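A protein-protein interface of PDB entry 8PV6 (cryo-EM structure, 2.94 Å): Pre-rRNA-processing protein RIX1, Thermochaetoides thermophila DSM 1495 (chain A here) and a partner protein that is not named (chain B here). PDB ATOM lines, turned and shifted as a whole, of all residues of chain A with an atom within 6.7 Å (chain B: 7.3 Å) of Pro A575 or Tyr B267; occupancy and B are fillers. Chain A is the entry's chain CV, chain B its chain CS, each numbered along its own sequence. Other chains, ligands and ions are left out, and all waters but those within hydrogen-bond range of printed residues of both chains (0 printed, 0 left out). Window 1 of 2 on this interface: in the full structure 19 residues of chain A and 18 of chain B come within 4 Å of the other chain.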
ATOM      1  N   PRO A 539      10.915 -18.675 -21.323  1.00  0.00           N
ATOM      2  CA  PRO A 539      10.205 -18.867 -20.044  1.00  0.00           C
ATOM      3  C   PRO A 539       9.522 -17.620 -19.508  1.00  0.00           C
ATOM      4  O   PRO A 539       8.496 -17.734 -18.825  1.00  0.00           O
ATOM      5  CB  PRO A 539      11.317 -19.350 -19.103  1.00  0.00           C
ATOM      6  CG  PRO A 539      12.575 -18.853 -19.714  1.00  0.00           C
ATOM      7  CD  PRO A 539      12.360 -18.923 -21.191  1.00  0.00           C
ATOM      8  N   ARG A 542       6.098 -17.430 -21.037  1.00  0.00           N
ATOM      9  CA  ARG A 542       5.188 -18.366 -20.380  1.00  0.00           C
ATOM     10  C   ARG A 542       4.743 -17.848 -19.019  1.00  0.00           C
ATOM     11  O   ARG A 542       3.567 -17.971 -18.652  1.00  0.00           O
ATOM     12  CB  ARG A 542       5.861 -19.731 -20.241  1.00  0.00           C
ATOM     13  CG  ARG A 542       4.988 -20.815 -19.627  1.00  0.00           C
ATOM     14  CD  ARG A 542       3.636 -20.922 -20.310  1.00  0.00           C
ATOM     15  NE  ARG A 542       2.764 -21.867 -19.626  1.00  0.00           N
ATOM     16  CZ  ARG A 542       2.496 -23.089 -20.063  1.00  0.00           C
ATOM     17  NH1 ARG A 542       3.011 -23.548 -21.190  1.00  0.00           N
ATOM     18  NH2 ARG A 542       1.690 -23.870 -19.350  1.00  0.00           N
ATOM     19  N   GLY A 543       5.670 -17.260 -18.259  1.00  0.00           N
ATOM     20  CA  GLY A 543       5.306 -16.679 -16.976  1.00  0.00           C
ATOM     21  C   GLY A 543       4.354 -15.507 -17.113  1.00  0.00           C
ATOM     22  O   GLY A 543       3.418 -15.364 -16.325  1.00  0.00           O
ATOM     23  N   LEU A 544       4.574 -14.662 -18.124  1.00  0.00           N
ATOM     24  CA  LEU A 544       3.668 -13.547 -18.386  1.00  0.00           C
ATOM     25  C   LEU A 544       2.284 -14.039 -18.790  1.00  0.00           C
ATOM     26  O   LEU A 544       1.271 -13.493 -18.340  1.00  0.00           O
ATOM     27  CB  LEU A 544       4.255 -12.646 -19.471  1.00  0.00           C
ATOM     28  CG  LEU A 544       3.373 -11.502 -19.967  1.00  0.00           C
ATOM     29  CD1 LEU A 544       3.087 -10.519 -18.848  1.00  0.00           C
ATOM     30  CD2 LEU A 544       4.019 -10.804 -21.147  1.00  0.00           C
ATOM     31  N   ASP A 546       0.870 -16.988 -18.005  1.00  0.00           N
ATOM     32  CA  ASP A 546       0.216 -17.587 -16.846  1.00  0.00           C
ATOM     33  C   ASP A 546      -0.225 -16.529 -15.840  1.00  0.00           C
ATOM     34  O   ASP A 546      -1.325 -16.620 -15.279  1.00  0.00           O
ATOM     35  CB  ASP A 546       1.151 -18.599 -16.191  1.00  0.00           C
ATOM     36  CG  ASP A 546       1.416 -19.798 -17.075  1.00  0.00           C
ATOM     37  OD1 ASP A 546       0.876 -19.836 -18.199  1.00  0.00           O
ATOM     38  OD2 ASP A 546       2.161 -20.704 -16.648  1.00  0.00           O
ATOM     39  N   ARG A 547       0.615 -15.514 -15.612  1.00  0.00           N
ATOM     40  CA  ARG A 547       0.251 -14.419 -14.721  1.00  0.00           C
ATOM     41  C   ARG A 547      -0.957 -13.661 -15.249  1.00  0.00           C
ATOM     42  O   ARG A 547      -1.858 -13.306 -14.481  1.00  0.00           O
ATOM     43  CB  ARG A 547       1.441 -13.475 -14.553  1.00  0.00           C
ATOM     44  CG  ARG A 547       1.247 -12.391 -13.513  1.00  0.00           C
ATOM     45  CD  ARG A 547       2.408 -11.409 -13.512  1.00  0.00           C
ATOM     46  NE  ARG A 547       3.682 -12.053 -13.223  1.00  0.00           N
ATOM     47  CZ  ARG A 547       4.691 -12.134 -14.080  1.00  0.00           C
ATOM     48  NH1 ARG A 547       4.610 -11.612 -15.293  1.00  0.00           N
ATOM     49  NH2 ARG A 547       5.809 -12.751 -13.710  1.00  0.00           N
ATOM     50  N   SER A 561      -3.382 -23.683 -20.109  1.00  0.00           N
ATOM     51  CA  SER A 561      -2.056 -23.723 -19.505  1.00  0.00           C
ATOM     52  C   SER A 561      -1.848 -25.004 -18.709  1.00  0.00           C
ATOM     53  O   SER A 561      -0.741 -25.552 -18.688  1.00  0.00           O
ATOM     54  CB  SER A 561      -1.848 -22.504 -18.613  1.00  0.00           C
ATOM     55  OG  SER A 561      -0.643 -22.621 -17.880  1.00  0.00           O
ATOM     56  N   TYR A 566       4.649 -26.393 -19.672  1.00  0.00           N
ATOM     57  CA  TYR A 566       5.911 -25.851 -20.166  1.00  0.00           C
ATOM     58  C   TYR A 566       7.059 -26.665 -19.585  1.00  0.00           C
ATOM     59  O   TYR A 566       7.216 -26.747 -18.362  1.00  0.00           O
ATOM     60  CB  TYR A 566       6.044 -24.376 -19.794  1.00  0.00           C
ATOM     61  CG  TYR A 566       7.302 -23.722 -20.312  1.00  0.00           C
ATOM     62  CD1 TYR A 566       7.378 -23.255 -21.615  1.00  0.00           C
ATOM     63  CD2 TYR A 566       8.413 -23.563 -19.493  1.00  0.00           C
ATOM     64  CE1 TYR A 566       8.526 -22.655 -22.091  1.00  0.00           C
ATOM     65  CE2 TYR A 566       9.565 -22.966 -19.961  1.00  0.00           C
ATOM     66  CZ  TYR A 566       9.615 -22.513 -21.260  1.00  0.00           C
ATOM     67  OH  TYR A 566      10.761 -21.915 -21.729  1.00  0.00           O
ATOM     68  N   ARG A 572      11.833 -31.054 -17.110  1.00  0.00           N
ATOM     69  CA  ARG A 572      10.880 -31.156 -16.017  1.00  0.00           C
ATOM     70  C   ARG A 572       9.736 -30.175 -16.235  1.00  0.00           C
ATOM     71  O   ARG A 572       9.957 -29.013 -16.585  1.00  0.00           O
ATOM     72  CB  ARG A 572      11.570 -30.878 -14.680  1.00  0.00           C
ATOM     73  CG  ARG A 572      10.652 -30.935 -13.473  1.00  0.00           C
ATOM     74  CD  ARG A 572      10.120 -32.340 -13.252  1.00  0.00           C
ATOM     75  NE  ARG A 572       9.263 -32.417 -12.076  1.00  0.00           N
ATOM     76  CZ  ARG A 572       7.962 -32.156 -12.081  1.00  0.00           C
ATOM     77  NH1 ARG A 572       7.333 -31.801 -13.188  1.00  0.00           N
ATOM     78  NH2 ARG A 572       7.277 -32.255 -10.944  1.00  0.00           N
ATOM     79  N   TYR A 573       8.513 -30.652 -16.034  1.00  0.00           N
ATOM     80  CA  TYR A 573       7.343 -29.823 -16.259  1.00  0.00           C
ATOM     81  C   TYR A 573       7.206 -28.759 -15.172  1.00  0.00           C
ATOM     82  O   TYR A 573       7.530 -28.977 -14.002  1.00  0.00           O
ATOM     83  CB  TYR A 573       6.076 -30.674 -16.310  1.00  0.00           C
ATOM     84  CG  TYR A 573       6.047 -31.681 -17.436  1.00  0.00           C
ATOM     85  CD1 TYR A 573       6.589 -32.949 -17.282  1.00  0.00           C
ATOM     86  CD2 TYR A 573       5.477 -31.358 -18.657  1.00  0.00           C
ATOM     87  CE1 TYR A 573       6.559 -33.867 -18.314  1.00  0.00           C
ATOM     88  CE2 TYR A 573       5.440 -32.266 -19.693  1.00  0.00           C
ATOM     89  CZ  TYR A 573       5.982 -33.520 -19.516  1.00  0.00           C
ATOM     90  OH  TYR A 573       5.950 -34.429 -20.548  1.00  0.00           O
ATOM     91  N   TYR A 574       6.728 -27.592 -15.586  1.00  0.00           N
ATOM     92  CA  TYR A 574       6.404 -26.515 -14.668  1.00  0.00           C
ATOM     93  C   TYR A 574       5.176 -26.877 -13.840  1.00  0.00           C
ATOM     94  O   TYR A 574       4.342 -27.677 -14.271  1.00  0.00           O
ATOM     95  CB  TYR A 574       6.158 -25.227 -15.447  1.00  0.00           C
ATOM     96  CG  TYR A 574       7.383 -24.354 -15.597  1.00  0.00           C
ATOM     97  CD1 TYR A 574       8.645 -24.914 -15.724  1.00  0.00           C
ATOM     98  CD2 TYR A 574       7.274 -22.971 -15.623  1.00  0.00           C
ATOM     99  CE1 TYR A 574       9.766 -24.120 -15.863  1.00  0.00           C
ATOM    100  CE2 TYR A 574       8.388 -22.170 -15.764  1.00  0.00           C
ATOM    101  CZ  TYR A 574       9.631 -22.750 -15.884  1.00  0.00           C
ATOM    102  OH  TYR A 574      10.744 -21.955 -16.024  1.00  0.00           O
ATOM    103  N   PRO A 575       5.060 -26.330 -12.627  1.00  0.00           N
ATOM    104  CA  PRO A 575       3.863 -26.582 -11.816  1.00  0.00           C
ATOM    105  C   PRO A 575       2.605 -26.032 -12.472  1.00  0.00           C
ATOM    106  O   PRO A 575       2.634 -25.023 -13.179  1.00  0.00           O
ATOM    107  CB  PRO A 575       4.169 -25.859 -10.501  1.00  0.00           C
ATOM    108  CG  PRO A 575       5.651 -25.829 -10.434  1.00  0.00           C
ATOM    109  CD  PRO A 575       6.110 -25.650 -11.849  1.00  0.00           C
ATOM    110  N   SER A 576       1.490 -26.714 -12.225  1.00  0.00           N
ATOM    111  CA  SER A 576       0.245 -26.421 -12.918  1.00  0.00           C
ATOM    112  C   SER A 576      -0.514 -25.286 -12.242  1.00  0.00           C
ATOM    113  O   SER A 576      -0.476 -25.133 -11.019  1.00  0.00           O
ATOM    114  CB  SER A 576      -0.630 -27.671 -12.978  1.00  0.00           C
ATOM    115  OG  SER A 576      -1.890 -27.381 -13.549  1.00  0.00           O
ATOM    116  N   ILE A 577      -1.219 -24.499 -13.060  1.00  0.00           N
ATOM    117  CA  ILE A 577      -2.023 -23.373 -12.581  1.00  0.00           C
ATOM    118  C   ILE A 577      -3.185 -23.851 -11.720  1.00  0.00           C
ATOM    119  O   ILE A 577      -3.618 -23.143 -10.800  1.00  0.00           O
ATOM    120  CB  ILE A 577      -2.486 -22.536 -13.800  1.00  0.00           C
ATOM    121  CG1 ILE A 577      -1.321 -21.705 -14.338  1.00  0.00           C
ATOM    122  CG2 ILE A 577      -3.680 -21.627 -13.496  1.00  0.00           C
ATOM    123  CD1 ILE A 577      -1.726 -20.703 -15.393  1.00  0.00           C
ATOM    124  N   LEU A 578      -3.636 -25.099 -11.936  1.00  0.00           N
ATOM    125  CA  LEU A 578      -4.836 -25.770 -11.423  1.00  0.00           C
ATOM    126  C   LEU A 578      -5.280 -25.422  -9.997  1.00  0.00           C
ATOM    127  O   LEU A 578      -6.496 -25.331  -9.771  1.00  0.00           O
ATOM    128  CB  LEU A 578      -4.659 -27.288 -11.550  1.00  0.00           C
ATOM    129  CG  LEU A 578      -5.921 -28.130 -11.374  1.00  0.00           C
ATOM    130  CD1 LEU A 578      -7.009 -27.654 -12.314  1.00  0.00           C
ATOM    131  CD2 LEU A 578      -5.619 -29.597 -11.596  1.00  0.00           C
ATOM    132  N   PRO A 579      -4.367 -25.246  -8.988  1.00  0.00           N
ATOM    133  CA  PRO A 579      -4.825 -24.696  -7.703  1.00  0.00           C
ATOM    134  C   PRO A 579      -5.558 -23.368  -7.821  1.00  0.00           C
ATOM    135  O   PRO A 579      -6.527 -23.136  -7.098  1.00  0.00           O
ATOM    136  CB  PRO A 579      -3.523 -24.531  -6.915  1.00  0.00           C
ATOM    137  CG  PRO A 579      -2.683 -25.620  -7.395  1.00  0.00           C
ATOM    138  CD  PRO A 579      -2.986 -25.760  -8.859  1.00  0.00           C
ATOM    139  N   PRO B 177      15.456 -15.731  -8.177  1.00  0.00           N
ATOM    140  CA  PRO B 177      15.321 -14.310  -8.537  1.00  0.00           C
ATOM    141  C   PRO B 177      16.400 -13.427  -7.930  1.00  0.00           C
ATOM    142  O   PRO B 177      16.559 -13.373  -6.707  1.00  0.00           O
ATOM    143  CB  PRO B 177      13.936 -13.941  -7.989  1.00  0.00           C
ATOM    144  CG  PRO B 177      13.197 -15.219  -7.956  1.00  0.00           C
ATOM    145  CD  PRO B 177      14.210 -16.261  -7.594  1.00  0.00           C
ATOM    146  N   ASN B 254       1.862 -34.359 -13.114  1.00  0.00           N
ATOM    147  CA  ASN B 254       1.985 -32.912 -13.005  1.00  0.00           C
ATOM    148  C   ASN B 254       0.646 -32.218 -12.782  1.00  0.00           C
ATOM    149  O   ASN B 254       0.625 -31.106 -12.247  1.00  0.00           O
ATOM    150  CB  ASN B 254       2.651 -32.354 -14.266  1.00  0.00           C
ATOM    151  CG  ASN B 254       3.122 -30.925 -14.097  1.00  0.00           C
ATOM    152  OD1 ASN B 254       3.664 -30.556 -13.056  1.00  0.00           O
ATOM    153  ND2 ASN B 254       2.916 -30.111 -15.122  1.00  0.00           N
ATOM    154  N   LEU B 258       0.699 -33.109  -6.170  1.00  0.00           N
ATOM    155  CA  LEU B 258       1.205 -31.856  -5.639  1.00  0.00           C
ATOM    156  C   LEU B 258       2.529 -31.486  -6.308  1.00  0.00           C
ATOM    157  O   LEU B 258       3.273 -32.364  -6.752  1.00  0.00           O
ATOM    158  CB  LEU B 258       1.400 -31.957  -4.130  1.00  0.00           C
ATOM    159  CG  LEU B 258       0.146 -32.031  -3.261  1.00  0.00           C
ATOM    160  CD1 LEU B 258       0.542 -32.228  -1.813  1.00  0.00           C
ATOM    161  CD2 LEU B 258      -0.695 -30.781  -3.420  1.00  0.00           C
ATOM    162  N   PRO B 259       2.834 -30.192  -6.411  1.00  0.00           N
ATOM    163  CA  PRO B 259       4.116 -29.785  -6.999  1.00  0.00           C
ATOM    164  C   PRO B 259       5.285 -30.174  -6.106  1.00  0.00           C
ATOM    165  O   PRO B 259       5.354 -29.787  -4.938  1.00  0.00           O
ATOM    166  CB  PRO B 259       3.980 -28.262  -7.120  1.00  0.00           C
ATOM    167  CG  PRO B 259       2.510 -28.013  -7.127  1.00  0.00           C
ATOM    168  CD  PRO B 259       1.943 -29.040  -6.201  1.00  0.00           C
ATOM    169  N   THR B 260       6.208 -30.949  -6.670  1.00  0.00           N
ATOM    170  CA  THR B 260       7.386 -31.413  -5.951  1.00  0.00           C
ATOM    171  C   THR B 260       8.573 -30.470  -6.086  1.00  0.00           C
ATOM    172  O   THR B 260       9.575 -30.655  -5.390  1.00  0.00           O
ATOM    173  CB  THR B 260       7.786 -32.807  -6.440  1.00  0.00           C
ATOM    174  OG1 THR B 260       8.220 -32.731  -7.802  1.00  0.00           O
ATOM    175  CG2 THR B 260       6.605 -33.760  -6.346  1.00  0.00           C
ATOM    176  N   THR B 261       8.486 -29.472  -6.960  1.00  0.00           N
ATOM    177  CA  THR B 261       9.570 -28.511  -7.116  1.00  0.00           C
ATOM    178  C   THR B 261       9.599 -27.553  -5.929  1.00  0.00           C
ATOM    179  O   THR B 261       8.560 -27.001  -5.555  1.00  0.00           O
ATOM    180  CB  THR B 261       9.407 -27.713  -8.405  1.00  0.00           C
ATOM    181  OG1 THR B 261       8.281 -26.836  -8.288  1.00  0.00           O
ATOM    182  CG2 THR B 261       9.194 -28.649  -9.585  1.00  0.00           C
ATOM    183  N   ASN B 263       9.800 -24.317  -3.798  1.00  0.00           N
ATOM    184  CA  ASN B 263       9.271 -22.990  -4.091  1.00  0.00           C
ATOM    185  C   ASN B 263       8.594 -22.927  -5.465  1.00  0.00           C
ATOM    186  O   ASN B 263       9.142 -22.349  -6.406  1.00  0.00           O
ATOM    187  CB  ASN B 263      10.358 -21.929  -3.982  1.00  0.00           C
ATOM    188  CG  ASN B 263       9.809 -20.512  -4.052  1.00  0.00           C
ATOM    189  OD1 ASN B 263       8.611 -20.284  -3.881  1.00  0.00           O
ATOM    190  ND2 ASN B 263      10.688 -19.552  -4.310  1.00  0.00           N
ATOM    191  N   PRO B 264       7.418 -23.533  -5.620  1.00  0.00           N
ATOM    192  CA  PRO B 264       6.707 -23.427  -6.893  1.00  0.00           C
ATOM    193  C   PRO B 264       6.043 -22.068  -7.027  1.00  0.00           C
ATOM    194  O   PRO B 264       5.883 -21.327  -6.055  1.00  0.00           O
ATOM    195  CB  PRO B 264       5.673 -24.550  -6.813  1.00  0.00           C
ATOM    196  CG  PRO B 264       5.361 -24.633  -5.373  1.00  0.00           C
ATOM    197  CD  PRO B 264       6.625 -24.274  -4.622  1.00  0.00           C
ATOM    198  N   PHE B 265       5.680 -21.745  -8.270  1.00  0.00           N
ATOM    199  CA  PHE B 265       5.012 -20.503  -8.656  1.00  0.00           C
ATOM    200  C   PHE B 265       5.819 -19.261  -8.304  1.00  0.00           C
ATOM    201  O   PHE B 265       5.246 -18.183  -8.116  1.00  0.00           O
ATOM    202  CB  PHE B 265       3.609 -20.406  -8.045  1.00  0.00           C
ATOM    203  CG  PHE B 265       2.794 -21.649  -8.223  1.00  0.00           C
ATOM    204  CD1 PHE B 265       2.262 -21.970  -9.456  1.00  0.00           C
ATOM    205  CD2 PHE B 265       2.570 -22.503  -7.158  1.00  0.00           C
ATOM    206  CE1 PHE B 265       1.519 -23.114  -9.623  1.00  0.00           C
ATOM    207  CE2 PHE B 265       1.823 -23.650  -7.322  1.00  0.00           C
ATOM    208  CZ  PHE B 265       1.298 -23.955  -8.556  1.00  0.00           C
ATOM    209  N   ALA B 266       7.144 -19.384  -8.205  1.00  0.00           N
ATOM    210  CA  ALA B 266       7.978 -18.210  -7.982  1.00  0.00           C
ATOM    211  C   ALA B 266       8.115 -17.378  -9.248  1.00  0.00           C
ATOM    212  O   ALA B 266       8.377 -16.174  -9.173  1.00  0.00           O
ATOM    213  CB  ALA B 266       9.355 -18.629  -7.469  1.00  0.00           C
ATOM    214  N   TYR B 267       7.945 -18.002 -10.416  1.00  0.00           N
ATOM    215  CA  TYR B 267       8.009 -17.266 -11.671  1.00  0.00           C
ATOM    216  C   TYR B 267       6.777 -16.402 -11.893  1.00  0.00           C
ATOM    217  O   TYR B 267       6.840 -15.442 -12.668  1.00  0.00           O
ATOM    218  CB  TYR B 267       8.199 -18.230 -12.848  1.00  0.00           C
ATOM    219  CG  TYR B 267       7.165 -19.334 -12.961  1.00  0.00           C
ATOM    220  CD1 TYR B 267       7.303 -20.519 -12.249  1.00  0.00           C
ATOM    221  CD2 TYR B 267       6.061 -19.195 -13.792  1.00  0.00           C
ATOM    222  CE1 TYR B 267       6.367 -21.528 -12.353  1.00  0.00           C
ATOM    223  CE2 TYR B 267       5.120 -20.202 -13.903  1.00  0.00           C
ATOM    224  CZ  TYR B 267       5.278 -21.362 -13.181  1.00  0.00           C
ATOM    225  OH  TYR B 267       4.343 -22.366 -13.287  1.00  0.00           O
ATOM    226  N   LEU B 268       5.661 -16.722 -11.240  1.00  0.00           N
ATOM    227  CA  LEU B 268       4.462 -15.903 -11.374  1.00  0.00           C
ATOM    228  C   LEU B 268       4.610 -14.564 -10.667  1.00  0.00           C
ATOM    229  O   LEU B 268       4.159 -13.538 -11.191  1.00  0.00           O
ATOM    230  CB  LEU B 268       3.249 -16.656 -10.833  1.00  0.00           C
ATOM    231  CG  LEU B 268       2.953 -17.979 -11.530  1.00  0.00           C
ATOM    232  CD1 LEU B 268       1.760 -18.664 -10.898  1.00  0.00           C
ATOM    233  CD2 LEU B 268       2.702 -17.717 -12.992  1.00  0.00           C
ATOM    234  N   ASN B 269       5.245 -14.565  -9.487  1.00  0.00           N
ATOM    235  CA  ASN B 269       5.430 -13.375  -8.648  1.00  0.00           C
ATOM    236  C   ASN B 269       4.097 -12.703  -8.329  1.00  0.00           C
ATOM    237  O   ASN B 269       3.961 -11.480  -8.392  1.00  0.00           O
ATOM    238  CB  ASN B 269       6.407 -12.385  -9.292  1.00  0.00           C
ATOM    239  CG  ASN B 269       7.026 -11.440  -8.286  1.00  0.00           C
ATOM    240  OD1 ASN B 269       7.251 -11.802  -7.131  1.00  0.00           O
ATOM    241  ND2 ASN B 269       7.303 -10.216  -8.718  1.00  0.00           N
ATOM    242  N   LEU B 270       3.092 -13.518  -8.001  1.00  0.00           N
ATOM    243  CA  LEU B 270       1.771 -12.976  -7.713  1.00  0.00           C
ATOM    244  C   LEU B 270       1.734 -12.298  -6.350  1.00  0.00           C
ATOM    245  O   LEU B 270       1.153 -11.216  -6.204  1.00  0.00           O
ATOM    246  CB  LEU B 270       0.723 -14.084  -7.790  1.00  0.00           C
ATOM    247  CG  LEU B 270       0.517 -14.737  -9.157  1.00  0.00           C
ATOM    248  CD1 LEU B 270      -0.407 -15.931  -9.043  1.00  0.00           C
ATOM    249  CD2 LEU B 270      -0.029 -13.732 -10.153  1.00  0.00           C
ATOM    250  N   ARG B 275       9.436  -7.092 -10.035  1.00  0.00           N
ATOM    251  CA  ARG B 275      10.856  -7.356 -10.216  1.00  0.00           C
ATOM    252  C   ARG B 275      11.407  -6.504 -11.348  1.00  0.00           C
ATOM    253  O   ARG B 275      10.808  -6.429 -12.425  1.00  0.00           O
ATOM    254  CB  ARG B 275      11.101  -8.837 -10.510  1.00  0.00           C
ATOM    255  CG  ARG B 275      10.669  -9.775  -9.400  1.00  0.00           C
ATOM    256  CD  ARG B 275      10.813 -11.223  -9.829  1.00  0.00           C
ATOM    257  NE  ARG B 275      10.228 -12.145  -8.863  1.00  0.00           N
ATOM    258  CZ  ARG B 275      10.082 -13.446  -9.066  1.00  0.00           C
ATOM    259  NH1 ARG B 275      10.466 -14.016 -10.195  1.00  0.00           N
ATOM    260  NH2 ARG B 275       9.536 -14.194  -8.112  1.00  0.00           N
ATOM    261  N   GLU B 280      14.985 -10.074 -11.719  1.00  0.00           N
ATOM    262  CA  GLU B 280      14.208 -11.027 -12.499  1.00  0.00           C
ATOM    263  C   GLU B 280      14.809 -12.425 -12.421  1.00  0.00           C
ATOM    264  O   GLU B 280      15.958 -12.616 -12.013  1.00  0.00           O
ATOM    265  CB  GLU B 280      14.118 -10.587 -13.961  1.00  0.00           C
ATOM    266  CG  GLU B 280      12.853  -9.820 -14.314  1.00  0.00           C
ATOM    267  CD  GLU B 280      11.649 -10.721 -14.517  1.00  0.00           C
ATOM    268  OE1 GLU B 280      11.821 -11.958 -14.552  1.00  0.00           O
ATOM    269  OE2 GLU B 280      10.526 -10.189 -14.641  1.00  0.00           O
ATOM    270  N   MET B 281      14.006 -13.407 -12.819  1.00  0.00           N
ATOM    271  CA  MET B 281      14.427 -14.798 -12.871  1.00  0.00           C
ATOM    272  C   MET B 281      14.958 -15.120 -14.262  1.00  0.00           C
ATOM    273  O   MET B 281      14.310 -14.811 -15.267  1.00  0.00           O
ATOM    274  CB  MET B 281      13.255 -15.718 -12.530  1.00  0.00           C
ATOM    275  CG  MET B 281      13.616 -17.186 -12.443  1.00  0.00           C
ATOM    276  SD  MET B 281      12.209 -18.235 -12.031  1.00  0.00           S
ATOM    277  CE  MET B 281      11.958 -17.816 -10.310  1.00  0.00           C
ATOM    278  N   PRO B 283      16.100 -18.572 -15.519  1.00  0.00           N
ATOM    279  CA  PRO B 283      16.340 -19.985 -15.192  1.00  0.00           C
ATOM    280  C   PRO B 283      17.215 -20.712 -16.200  1.00  0.00           C
ATOM    281  O   PRO B 283      18.080 -21.502 -15.811  1.00  0.00           O
ATOM    282  CB  PRO B 283      14.925 -20.579 -15.159  1.00  0.00           C
ATOM    283  CG  PRO B 283      14.113 -19.683 -16.019  1.00  0.00           C
ATOM    284  CD  PRO B 283      14.701 -18.312 -15.897  1.00  0.00           C
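Pro A575 touches four residues of chain B. Tyr B267 touches just these residues of chain A: Arg A547 (3.1 Å), Tyr A574 (3.5 Å) and Pro A575 (3.2 Å). Printed residues of chain A within 4 Å of Thr B261: Pro A575 (3.5 Å). Of the printed residues of chain A, Pro B264 touches Pro A575. Ser A561 touches none of the printed residues of chain B. Tyr A566 touches none of the printed residues of chain B. The nearest printed residue of chain B that does not touch Pro A575 is Pro B259 (4.2 Å).
Leu B268 touches Asp A546. Arg A547 touches Leu B270 (CG to CD2, 3.8 Å). Asn B254 touches Arg A572. Tyr A573 touches Asn B254. CD2 of Tyr A574 touches CZ of Tyr B267 (3.5 Å). Pro A575 touches Thr B261. CG of Pro A575 touches CB of Pro B264, 3.8 Å away. Pro A575 touches Phe B265. Ser A576 touches Asn B254. Phe B265 touches Ser A576 (CE1 to O, 3.2 Å).
Hydrophobic or aromatic side chains of chain B within 4 Å of the printed part of chain A: Pro B264, Phe B265, Tyr B267, Leu B268 and Leu B270. Of the 16 printed residues of chain A, 7 touch a printed residue of chain B. Printed residues of chain A that touch a printed residue of chain B: Asp A546, Arg A547, Arg A572, Tyr A573, Tyr A574, Pro A575 and Ser A576. Hydrophobic or aromatic side chains of chain A within 4 Å of the printed part of chain B: Tyr A573, Tyr A574 and Pro A575. Along chain A the printed residues that touch a printed residue of chain B span positions 546 to 576.
NE of Arg A547 is in hydrogen-bond range of O of Leu B268 (2.6 Å). NH2 of Arg A547 sits at hydrogen-bond distance from O of Tyr B267 (3.1 Å). The side-chain hydroxyl (OH) of Tyr B267 lies within hydrogen-bond range of the backbone carbonyl oxygen (O) of Pro A575 (3.2 Å). ND2 of Asn B254 lies within hydrogen-bond range of O of Tyr A574, 2.9 Å away. OG1 of Thr B260 lies within hydrogen-bond range of NH2 of Arg A572 (3.3 Å).
The side-chain hydroxyl (OG) of Ser A561 lies within hydrogen-bond range of the side-chain carboxylate (OD1) of Asp A546, 3.2 Å away. The side-chain hydroxyl (OG) of Ser A576 sits close to the backbone NH (N) of Leu A578. N of Tyr A574 lies within hydrogen-bond range of O of Tyr A566 (2.9 Å). NE of Arg A542 is in salt-bridge range of OD1 of Asp A546, 3.1 Å away.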
